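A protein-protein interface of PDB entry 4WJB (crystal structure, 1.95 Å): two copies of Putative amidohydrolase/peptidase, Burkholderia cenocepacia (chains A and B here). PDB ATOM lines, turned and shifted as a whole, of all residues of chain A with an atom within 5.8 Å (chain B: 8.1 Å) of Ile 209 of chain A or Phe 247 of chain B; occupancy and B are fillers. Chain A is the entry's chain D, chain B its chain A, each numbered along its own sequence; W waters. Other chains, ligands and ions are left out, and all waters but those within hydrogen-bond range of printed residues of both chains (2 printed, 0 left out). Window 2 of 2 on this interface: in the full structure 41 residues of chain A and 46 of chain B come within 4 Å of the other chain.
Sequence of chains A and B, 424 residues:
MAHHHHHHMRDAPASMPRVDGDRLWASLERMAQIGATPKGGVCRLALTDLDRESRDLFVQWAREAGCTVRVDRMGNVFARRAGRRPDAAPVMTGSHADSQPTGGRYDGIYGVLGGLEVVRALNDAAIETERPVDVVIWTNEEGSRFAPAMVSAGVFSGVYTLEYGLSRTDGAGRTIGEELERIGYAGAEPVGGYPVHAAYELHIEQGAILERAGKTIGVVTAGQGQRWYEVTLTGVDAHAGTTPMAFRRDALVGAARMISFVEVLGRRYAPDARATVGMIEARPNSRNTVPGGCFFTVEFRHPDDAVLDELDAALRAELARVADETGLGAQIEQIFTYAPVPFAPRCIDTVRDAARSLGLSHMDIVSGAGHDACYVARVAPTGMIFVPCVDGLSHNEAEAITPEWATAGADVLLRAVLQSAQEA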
ATOM      1  N   GLU A 205      -3.948 -23.395  24.455  1.00  0.00           N
ATOM      2  CA  GLU A 205      -3.838 -22.578  25.659  1.00  0.00           C
ATOM      3  C   GLU A 205      -5.143 -22.505  26.458  1.00  0.00           C
ATOM      4  O   GLU A 205      -5.118 -22.426  27.691  1.00  0.00           O
ATOM      5  CB  GLU A 205      -3.385 -21.157  25.302  1.00  0.00           C
ATOM      6  CG  GLU A 205      -3.257 -20.241  26.522  1.00  0.00           C
ATOM      7  CD  GLU A 205      -3.180 -18.768  26.173  1.00  0.00           C
ATOM      8  OE1 GLU A 205      -2.674 -18.422  25.081  1.00  0.00           O
ATOM      9  OE2 GLU A 205      -3.623 -17.949  27.004  1.00  0.00           O
ATOM     10  N   GLY A 207      -6.985 -19.977  26.279  1.00  0.00           N
ATOM     11  CA  GLY A 207      -6.967 -18.586  26.691  1.00  0.00           C
ATOM     12  C   GLY A 207      -6.498 -17.724  25.534  1.00  0.00           C
ATOM     13  O   GLY A 207      -6.354 -18.213  24.413  1.00  0.00           O
ATOM     14  N   ALA A 208      -6.236 -16.448  25.802  1.00  0.00           N
ATOM     15  CA  ALA A 208      -5.914 -15.500  24.739  1.00  0.00           C
ATOM     16  C   ALA A 208      -4.518 -14.893  24.870  1.00  0.00           C
ATOM     17  O   ALA A 208      -4.178 -13.964  24.138  1.00  0.00           O
ATOM     18  CB  ALA A 208      -6.966 -14.379  24.708  1.00  0.00           C
ATOM     19  N   ILE A 209      -3.709 -15.406  25.792  1.00  0.00           N
ATOM     20  CA  ILE A 209      -2.417 -14.786  26.084  1.00  0.00           C
ATOM     21  C   ILE A 209      -1.468 -14.858  24.890  1.00  0.00           C
ATOM     22  O   ILE A 209      -0.938 -13.836  24.452  1.00  0.00           O
ATOM     23  CB  ILE A 209      -1.745 -15.430  27.313  1.00  0.00           C
ATOM     24  CG1 ILE A 209      -2.584 -15.173  28.574  1.00  0.00           C
ATOM     25  CG2 ILE A 209      -0.337 -14.887  27.497  1.00  0.00           C
ATOM     26  CD1 ILE A 209      -2.010 -15.796  29.830  1.00  0.00           C
ATOM     27  N   LEU A 210      -1.267 -16.061  24.361  1.00  0.00           N
ATOM     28  CA  LEU A 210      -0.381 -16.256  23.216  1.00  0.00           C
ATOM     29  C   LEU A 210      -0.867 -15.481  22.000  1.00  0.00           C
ATOM     30  O   LEU A 210      -0.088 -14.796  21.341  1.00  0.00           O
ATOM     31  CB  LEU A 210      -0.266 -17.737  22.871  1.00  0.00           C
ATOM     32  CG  LEU A 210       0.418 -18.611  23.920  1.00  0.00           C
ATOM     33  CD1 LEU A 210       0.431 -20.060  23.481  1.00  0.00           C
ATOM     34  CD2 LEU A 210       1.826 -18.112  24.173  1.00  0.00           C
ATOM     35  N   GLU A 211      -2.160 -15.593  21.715  1.00  0.00           N
ATOM     36  CA  GLU A 211      -2.757 -14.939  20.558  1.00  0.00           C
ATOM     37  C   GLU A 211      -2.578 -13.421  20.591  1.00  0.00           C
ATOM     38  O   GLU A 211      -2.156 -12.820  19.603  1.00  0.00           O
ATOM     39  CB  GLU A 211      -4.244 -15.283  20.466  1.00  0.00           C
ATOM     40  CG  GLU A 211      -4.868 -14.948  19.128  1.00  0.00           C
ATOM     41  CD  GLU A 211      -6.220 -14.294  19.271  1.00  0.00           C
ATOM     42  OE1 GLU A 211      -6.283 -13.183  19.842  1.00  0.00           O
ATOM     43  OE2 GLU A 211      -7.221 -14.889  18.817  1.00  0.00           O
ATOM     44  N   ARG A 212      -2.890 -12.803  21.725  1.00  0.00           N
ATOM     45  CA  ARG A 212      -2.780 -11.351  21.830  1.00  0.00           C
ATOM     46  C   ARG A 212      -1.329 -10.872  21.891  1.00  0.00           C
ATOM     47  O   ARG A 212      -1.027  -9.747  21.490  1.00  0.00           O
ATOM     48  CB  ARG A 212      -3.545 -10.840  23.055  1.00  0.00           C
ATOM     49  CG  ARG A 212      -5.041 -11.068  22.966  1.00  0.00           C
ATOM     50  CD  ARG A 212      -5.801 -10.265  23.999  1.00  0.00           C
ATOM     51  NE  ARG A 212      -7.204 -10.656  24.026  1.00  0.00           N
ATOM     52  CZ  ARG A 212      -8.160  -9.974  24.645  1.00  0.00           C
ATOM     53  NH1 ARG A 212      -7.871  -8.850  25.291  1.00  0.00           N
ATOM     54  NH2 ARG A 212      -9.411 -10.413  24.614  1.00  0.00           N
ATOM     55  N   ALA A 213      -0.439 -11.717  22.400  1.00  0.00           N
ATOM     56  CA  ALA A 213       0.979 -11.374  22.476  1.00  0.00           C
ATOM     57  C   ALA A 213       1.686 -11.672  21.158  1.00  0.00           C
ATOM     58  O   ALA A 213       2.849 -11.317  20.974  1.00  0.00           O
ATOM     59  CB  ALA A 213       1.653 -12.126  23.615  1.00  0.00           C
ATOM     60  N   GLY A 214       0.980 -12.335  20.249  1.00  0.00           N
ATOM     61  CA  GLY A 214       1.531 -12.670  18.950  1.00  0.00           C
ATOM     62  C   GLY A 214       2.618 -13.726  19.027  1.00  0.00           C
ATOM     63  O   GLY A 214       3.523 -13.764  18.190  1.00  0.00           O
ATOM     64  N   LYS A 215       2.530 -14.583  20.039  1.00  0.00           N
ATOM     65  CA  LYS A 215       3.508 -15.651  20.223  1.00  0.00           C
ATOM     66  C   LYS A 215       2.894 -17.001  19.874  1.00  0.00           C
ATOM     67  O   LYS A 215       1.779 -17.318  20.294  1.00  0.00           O
ATOM     68  CB  LYS A 215       4.036 -15.660  21.659  1.00  0.00           C
ATOM     69  CG  LYS A 215       4.670 -14.347  22.103  1.00  0.00           C
ATOM     70  CD  LYS A 215       5.916 -14.014  21.296  1.00  0.00           C
ATOM     71  CE  LYS A 215       6.542 -12.708  21.770  1.00  0.00           C
ATOM     72  NZ  LYS A 215       7.891 -12.479  21.183  1.00  0.00           N
ATOM     73  N   ARG A 274      -4.871 -14.328  39.432  1.00  0.00           N
ATOM     74  CA  ARG A 274      -6.270 -14.324  39.038  1.00  0.00           C
ATOM     75  C   ARG A 274      -7.105 -14.081  40.291  1.00  0.00           C
ATOM     76  O   ARG A 274      -6.953 -14.785  41.290  1.00  0.00           O
ATOM     77  CB  ARG A 274      -6.663 -15.641  38.364  1.00  0.00           C
ATOM     78  CG  ARG A 274      -5.735 -16.058  37.225  1.00  0.00           C
ATOM     79  CD  ARG A 274      -5.875 -15.153  36.014  1.00  0.00           C
ATOM     80  NE  ARG A 274      -5.084 -15.656  34.893  1.00  0.00           N
ATOM     81  CZ  ARG A 274      -3.864 -15.227  34.583  1.00  0.00           C
ATOM     82  NH1 ARG A 274      -3.294 -14.265  35.296  1.00  0.00           N
ATOM     83  NH2 ARG A 274      -3.217 -15.754  33.549  1.00  0.00           N
ATOM     84  N   MET A 363       7.010 -17.631  24.418  1.00  0.00           N
ATOM     85  CA  MET A 363       7.028 -16.914  25.684  1.00  0.00           C
ATOM     86  C   MET A 363       6.698 -17.873  26.817  1.00  0.00           C
ATOM     87  O   MET A 363       5.981 -18.855  26.617  1.00  0.00           O
ATOM     88  CB  MET A 363       6.028 -15.754  25.668  1.00  0.00           C
ATOM     89  CG  MET A 363       4.615 -16.176  25.312  1.00  0.00           C
ATOM     90  SD  MET A 363       3.398 -14.857  25.515  1.00  0.00           S
ATOM     91  CE  MET A 363       3.490 -14.577  27.279  1.00  0.00           C
ATOM     92  N   ILE A 365       4.682 -19.126  29.930  1.00  0.00           N
ATOM     93  CA  ILE A 365       3.275 -18.986  30.242  1.00  0.00           C
ATOM     94  C   ILE A 365       2.899 -19.910  31.394  1.00  0.00           C
ATOM     95  O   ILE A 365       3.522 -20.950  31.601  1.00  0.00           O
ATOM     96  CB  ILE A 365       2.389 -19.272  29.006  1.00  0.00           C
ATOM     97  CG1 ILE A 365       0.947 -18.817  29.262  1.00  0.00           C
ATOM     98  CG2 ILE A 365       2.468 -20.748  28.599  1.00  0.00           C
ATOM     99  CD1 ILE A 365       0.078 -18.792  28.029  1.00  0.00           C
ATOM    100  N   VAL A 366       1.906 -19.493  32.173  1.00  0.00           N
ATOM    101  CA  VAL A 366       1.361 -20.312  33.240  1.00  0.00           C
ATOM    102  C   VAL A 366       0.052 -20.928  32.762  1.00  0.00           C
ATOM    103  O   VAL A 366      -0.766 -20.243  32.148  1.00  0.00           O
ATOM    104  CB  VAL A 366       1.128 -19.477  34.522  1.00  0.00           C
ATOM    105  CG1 VAL A 366       0.421 -20.295  35.587  1.00  0.00           C
ATOM    106  CG2 VAL A 366       2.454 -18.934  35.044  1.00  0.00           C
ATOM    107  N   VAL B 236     -18.198 -10.175  29.201  1.00  0.00           N
ATOM    108  CA  VAL B 236     -17.780 -11.366  28.476  1.00  0.00           C
ATOM    109  C   VAL B 236     -17.589 -12.548  29.418  1.00  0.00           C
ATOM    110  O   VAL B 236     -16.760 -12.494  30.328  1.00  0.00           O
ATOM    111  CB  VAL B 236     -16.467 -11.119  27.708  1.00  0.00           C
ATOM    112  CG1 VAL B 236     -16.023 -12.382  26.986  1.00  0.00           C
ATOM    113  CG2 VAL B 236     -16.631  -9.970  26.727  1.00  0.00           C
ATOM    114  N   ALA B 238     -16.048 -15.616  30.820  1.00  0.00           N
ATOM    115  CA  ALA B 238     -14.662 -16.049  30.716  1.00  0.00           C
ATOM    116  C   ALA B 238     -14.255 -16.896  31.910  1.00  0.00           C
ATOM    117  O   ALA B 238     -14.609 -16.595  33.053  1.00  0.00           O
ATOM    118  CB  ALA B 238     -13.741 -14.849  30.584  1.00  0.00           C
ATOM    119  N   GLY B 241      -9.423 -18.770  35.606  1.00  0.00           N
ATOM    120  CA  GLY B 241      -8.033 -19.189  35.651  1.00  0.00           C
ATOM    121  C   GLY B 241      -7.226 -18.842  34.412  1.00  0.00           C
ATOM    122  O   GLY B 241      -6.046 -18.503  34.505  1.00  0.00           O
ATOM    123  N   THR B 242      -7.859 -18.924  33.248  1.00  0.00           N
ATOM    124  CA  THR B 242      -7.157 -18.736  31.983  1.00  0.00           C
ATOM    125  C   THR B 242      -7.229 -17.302  31.466  1.00  0.00           C
ATOM    126  O   THR B 242      -6.611 -16.975  30.453  1.00  0.00           O
ATOM    127  CB  THR B 242      -7.716 -19.670  30.896  1.00  0.00           C
ATOM    128  OG1 THR B 242      -9.124 -19.447  30.757  1.00  0.00           O
ATOM    129  CG2 THR B 242      -7.472 -21.130  31.264  1.00  0.00           C
ATOM    130  N   THR B 243      -7.980 -16.449  32.158  1.00  0.00           N
ATOM    131  CA  THR B 243      -8.184 -15.074  31.705  1.00  0.00           C
ATOM    132  C   THR B 243      -7.521 -14.046  32.622  1.00  0.00           C
ATOM    133  O   THR B 243      -8.022 -13.771  33.713  1.00  0.00           O
ATOM    134  CB  THR B 243      -9.686 -14.728  31.609  1.00  0.00           C
ATOM    135  OG1 THR B 243     -10.382 -15.761  30.900  1.00  0.00           O
ATOM    136  CG2 THR B 243      -9.875 -13.404  30.890  1.00  0.00           C
ATOM    137  N   PRO B 244      -6.396 -13.467  32.175  1.00  0.00           N
ATOM    138  CA  PRO B 244      -5.726 -12.398  32.925  1.00  0.00           C
ATOM    139  C   PRO B 244      -6.649 -11.205  33.154  1.00  0.00           C
ATOM    140  O   PRO B 244      -7.516 -10.939  32.322  1.00  0.00           O
ATOM    141  CB  PRO B 244      -4.557 -12.008  32.020  1.00  0.00           C
ATOM    142  CG  PRO B 244      -4.308 -13.219  31.179  1.00  0.00           C
ATOM    143  CD  PRO B 244      -5.662 -13.826  30.950  1.00  0.00           C
ATOM    144  N   MET B 245      -6.451 -10.504  34.267  1.00  0.00           N
ATOM    145  CA  MET B 245      -7.276  -9.360  34.634  1.00  0.00           C
ATOM    146  C   MET B 245      -7.421  -8.362  33.484  1.00  0.00           C
ATOM    147  O   MET B 245      -8.513  -7.871  33.213  1.00  0.00           O
ATOM    148  CB  MET B 245      -6.683  -8.666  35.862  1.00  0.00           C
ATOM    149  CG  MET B 245      -6.394  -9.609  37.020  1.00  0.00           C
ATOM    150  SD  MET B 245      -7.885 -10.404  37.662  1.00  0.00           S
ATOM    151  CE  MET B 245      -8.763  -9.007  38.387  1.00  0.00           C
ATOM    152  N   ALA B 246      -6.320  -8.095  32.793  1.00  0.00           N
ATOM    153  CA  ALA B 246      -6.303  -7.106  31.718  1.00  0.00           C
ATOM    154  C   ALA B 246      -7.211  -7.463  30.536  1.00  0.00           C
ATOM    155  O   ALA B 246      -7.541  -6.597  29.728  1.00  0.00           O
ATOM    156  CB  ALA B 246      -4.877  -6.900  31.227  1.00  0.00           C
ATOM    157  N   PHE B 247      -7.612  -8.728  30.433  1.00  0.00           N
ATOM    158  CA  PHE B 247      -8.463  -9.170  29.326  1.00  0.00           C
ATOM    159  C   PHE B 247      -9.946  -9.174  29.698  1.00  0.00           C
ATOM    160  O   PHE B 247     -10.807  -9.380  28.842  1.00  0.00           O
ATOM    161  CB  PHE B 247      -8.073 -10.580  28.862  1.00  0.00           C
ATOM    162  CG  PHE B 247      -6.681 -10.688  28.298  1.00  0.00           C
ATOM    163  CD1 PHE B 247      -5.918  -9.559  28.049  1.00  0.00           C
ATOM    164  CD2 PHE B 247      -6.141 -11.934  28.005  1.00  0.00           C
ATOM    165  CE1 PHE B 247      -4.635  -9.670  27.529  1.00  0.00           C
ATOM    166  CE2 PHE B 247      -4.862 -12.051  27.487  1.00  0.00           C
ATOM    167  CZ  PHE B 247      -4.109 -10.918  27.247  1.00  0.00           C
ATOM    168  N   ARG B 248     -10.238  -8.951  30.974  1.00  0.00           N
ATOM    169  CA  ARG B 248     -11.574  -9.203  31.507  1.00  0.00           C
ATOM    170  C   ARG B 248     -12.603  -8.107  31.237  1.00  0.00           C
ATOM    171  O   ARG B 248     -12.289  -6.915  31.241  1.00  0.00           O
ATOM    172  CB  ARG B 248     -11.485  -9.441  33.015  1.00  0.00           C
ATOM    173  CG  ARG B 248     -10.633 -10.641  33.387  1.00  0.00           C
ATOM    174  CD  ARG B 248     -10.755 -10.958  34.858  1.00  0.00           C
ATOM    175  NE  ARG B 248     -10.068 -12.198  35.203  1.00  0.00           N
ATOM    176  CZ  ARG B 248     -10.200 -12.809  36.375  1.00  0.00           C
ATOM    177  NH1 ARG B 248     -10.997 -12.295  37.304  1.00  0.00           N
ATOM    178  NH2 ARG B 248      -9.550 -13.936  36.617  1.00  0.00           N
ATOM    179  N   ARG B 249     -13.835  -8.544  30.999  1.00  0.00           N
ATOM    180  CA  ARG B 249     -14.994  -7.669  30.919  1.00  0.00           C
ATOM    181  C   ARG B 249     -15.996  -8.138  31.967  1.00  0.00           C
ATOM    182  O   ARG B 249     -17.033  -8.717  31.642  1.00  0.00           O
ATOM    183  CB  ARG B 249     -15.615  -7.688  29.521  1.00  0.00           C
ATOM    184  CG  ARG B 249     -14.716  -7.120  28.430  1.00  0.00           C
ATOM    185  CD  ARG B 249     -14.405  -5.655  28.690  1.00  0.00           C
ATOM    186  NE  ARG B 249     -13.644  -5.045  27.602  1.00  0.00           N
ATOM    187  CZ  ARG B 249     -12.317  -4.977  27.563  1.00  0.00           C
ATOM    188  NH1 ARG B 249     -11.590  -5.486  28.549  1.00  0.00           N
ATOM    189  NH2 ARG B 249     -11.716  -4.399  26.534  1.00  0.00           N
ATOM    190  N   ASP B 250     -15.658  -7.901  33.231  1.00  0.00           N
ATOM    191  CA  ASP B 250     -16.432  -8.413  34.355  1.00  0.00           C
ATOM    192  C   ASP B 250     -17.650  -7.538  34.632  1.00  0.00           C
ATOM    193  O   ASP B 250     -17.521  -6.416  35.120  1.00  0.00           O
ATOM    194  CB  ASP B 250     -15.543  -8.509  35.599  1.00  0.00           C
ATOM    195  CG  ASP B 250     -16.169  -9.335  36.713  1.00  0.00           C
ATOM    196  OD1 ASP B 250     -17.402  -9.248  36.918  1.00  0.00           O
ATOM    197  OD2 ASP B 250     -15.415 -10.054  37.404  1.00  0.00           O
ATOM    198  N   VAL B 290     -15.619 -15.471  35.223  1.00  0.00           N
ATOM    199  CA  VAL B 290     -15.849 -14.038  35.199  1.00  0.00           C
ATOM    200  C   VAL B 290     -17.254 -13.775  34.678  1.00  0.00           C
ATOM    201  O   VAL B 290     -17.574 -14.172  33.557  1.00  0.00           O
ATOM    202  CB  VAL B 290     -14.822 -13.318  34.305  1.00  0.00           C
ATOM    203  CG1 VAL B 290     -15.118 -11.826  34.251  1.00  0.00           C
ATOM    204  CG2 VAL B 290     -13.398 -13.595  34.788  1.00  0.00           C
ATOM    205  N   THR B 326     -14.843   0.524  31.712  1.00  0.00           N
ATOM    206  CA  THR B 326     -14.753  -0.916  31.919  1.00  0.00           C
ATOM    207  C   THR B 326     -14.865  -1.692  30.611  1.00  0.00           C
ATOM    208  O   THR B 326     -14.457  -2.852  30.531  1.00  0.00           O
ATOM    209  CB  THR B 326     -15.841  -1.415  32.885  1.00  0.00           C
ATOM    210  OG1 THR B 326     -17.132  -1.091  32.358  1.00  0.00           O
ATOM    211  CG2 THR B 326     -15.680  -0.767  34.255  1.00  0.00           C
HETATM  212  O   HOH W   1      -4.473 -18.561  29.671  1.00  0.00           O
HETATM  213  O   HOH W   2      -7.137 -15.644  28.332  1.00  0.00           O
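Of the 14 printed residues of chain B, 5 touch a printed residue of chain A. Among the printed residues, 8 pairs touch across the chains. Among the printed residues, no Asp or Glu carboxylate lies within 4 Å of a Lys or Arg side-chain nitrogen of the other chain.
Water W2 lies within hydrogen-bond range of O of Thr 242 of chain B (2.6 Å) and N of Ala 208 of chain A (2.8 Å). Water W1 lies within hydrogen-bond range of the backbone carbonyl oxygen of Thr 242 of chain B (2.8 Å) and the side-chain carboxylate of Glu 205 of chain A (2.9 Å).
Ala 208 of chain A touches one residue of chain B. Printed residues of chain B within 4 Å of Arg 212 of chain A: Phe 247. Printed residues of chain B within 4 Å of Arg 274 of chain A: Gly 241, Thr 243, Pro 244 and Arg 248. Of the printed residues of chain A, Gly 241 of chain B touches Arg 274 (3.0 Å). Of the printed residues of chain A, Phe 247 of chain B touches Ala 208 (3.9 Å), Ile 209 (3.9 Å) and Arg 212 (3.5 Å). Of the printed residues of chain A, Arg 248 of chain B touches Arg 274 (3.8 Å). The nearest printed residue of chain A that does not touch Phe 247 of chain B is Glu 205 of chain A (6.0 Å).
No position is printed for both chains.
Among the printed residues, merely in contact across the chains: Ala 208 of chain A with Phe 247 of chain B (3.9 Å), Ile 209 of chain A with Pro 244 of chain B (3.7 Å), Ile 209 of chain A with Phe 247 of chain B (3.9 Å), Arg 212 of chain A with Phe 247 of chain B (3.5 Å), Arg 274 of chain A with Thr 243 of chain B (3.4 Å), Arg 274 of chain A with Pro 244 of chain B (3.6 Å) and Arg 274 of chain A with Arg 248 of chain B (3.8 Å).
The side-chain sulfur (SD) of Met 245 of chain B sits close to the guanidinium group (NH1) of Arg 248 of chain B (3.7 Å). N of Ala 208 of chain A is in hydrogen-bond range of OE2 of Glu 205 of chain A, at 3.2 Å. The side-chain carboxylate (OE2) of Glu 205 of chain A sits at hydrogen-bond distance from the backbone NH (N) of Ile 209 of chain A (2.8 Å). NE of Arg 248 of chain B sits at hydrogen-bond distance from O of Thr 243 of chain B (3.0 Å).
O of Gly 241 of chain B sits at hydrogen-bond distance from NE of Arg 274 of chain A (3.0 Å).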
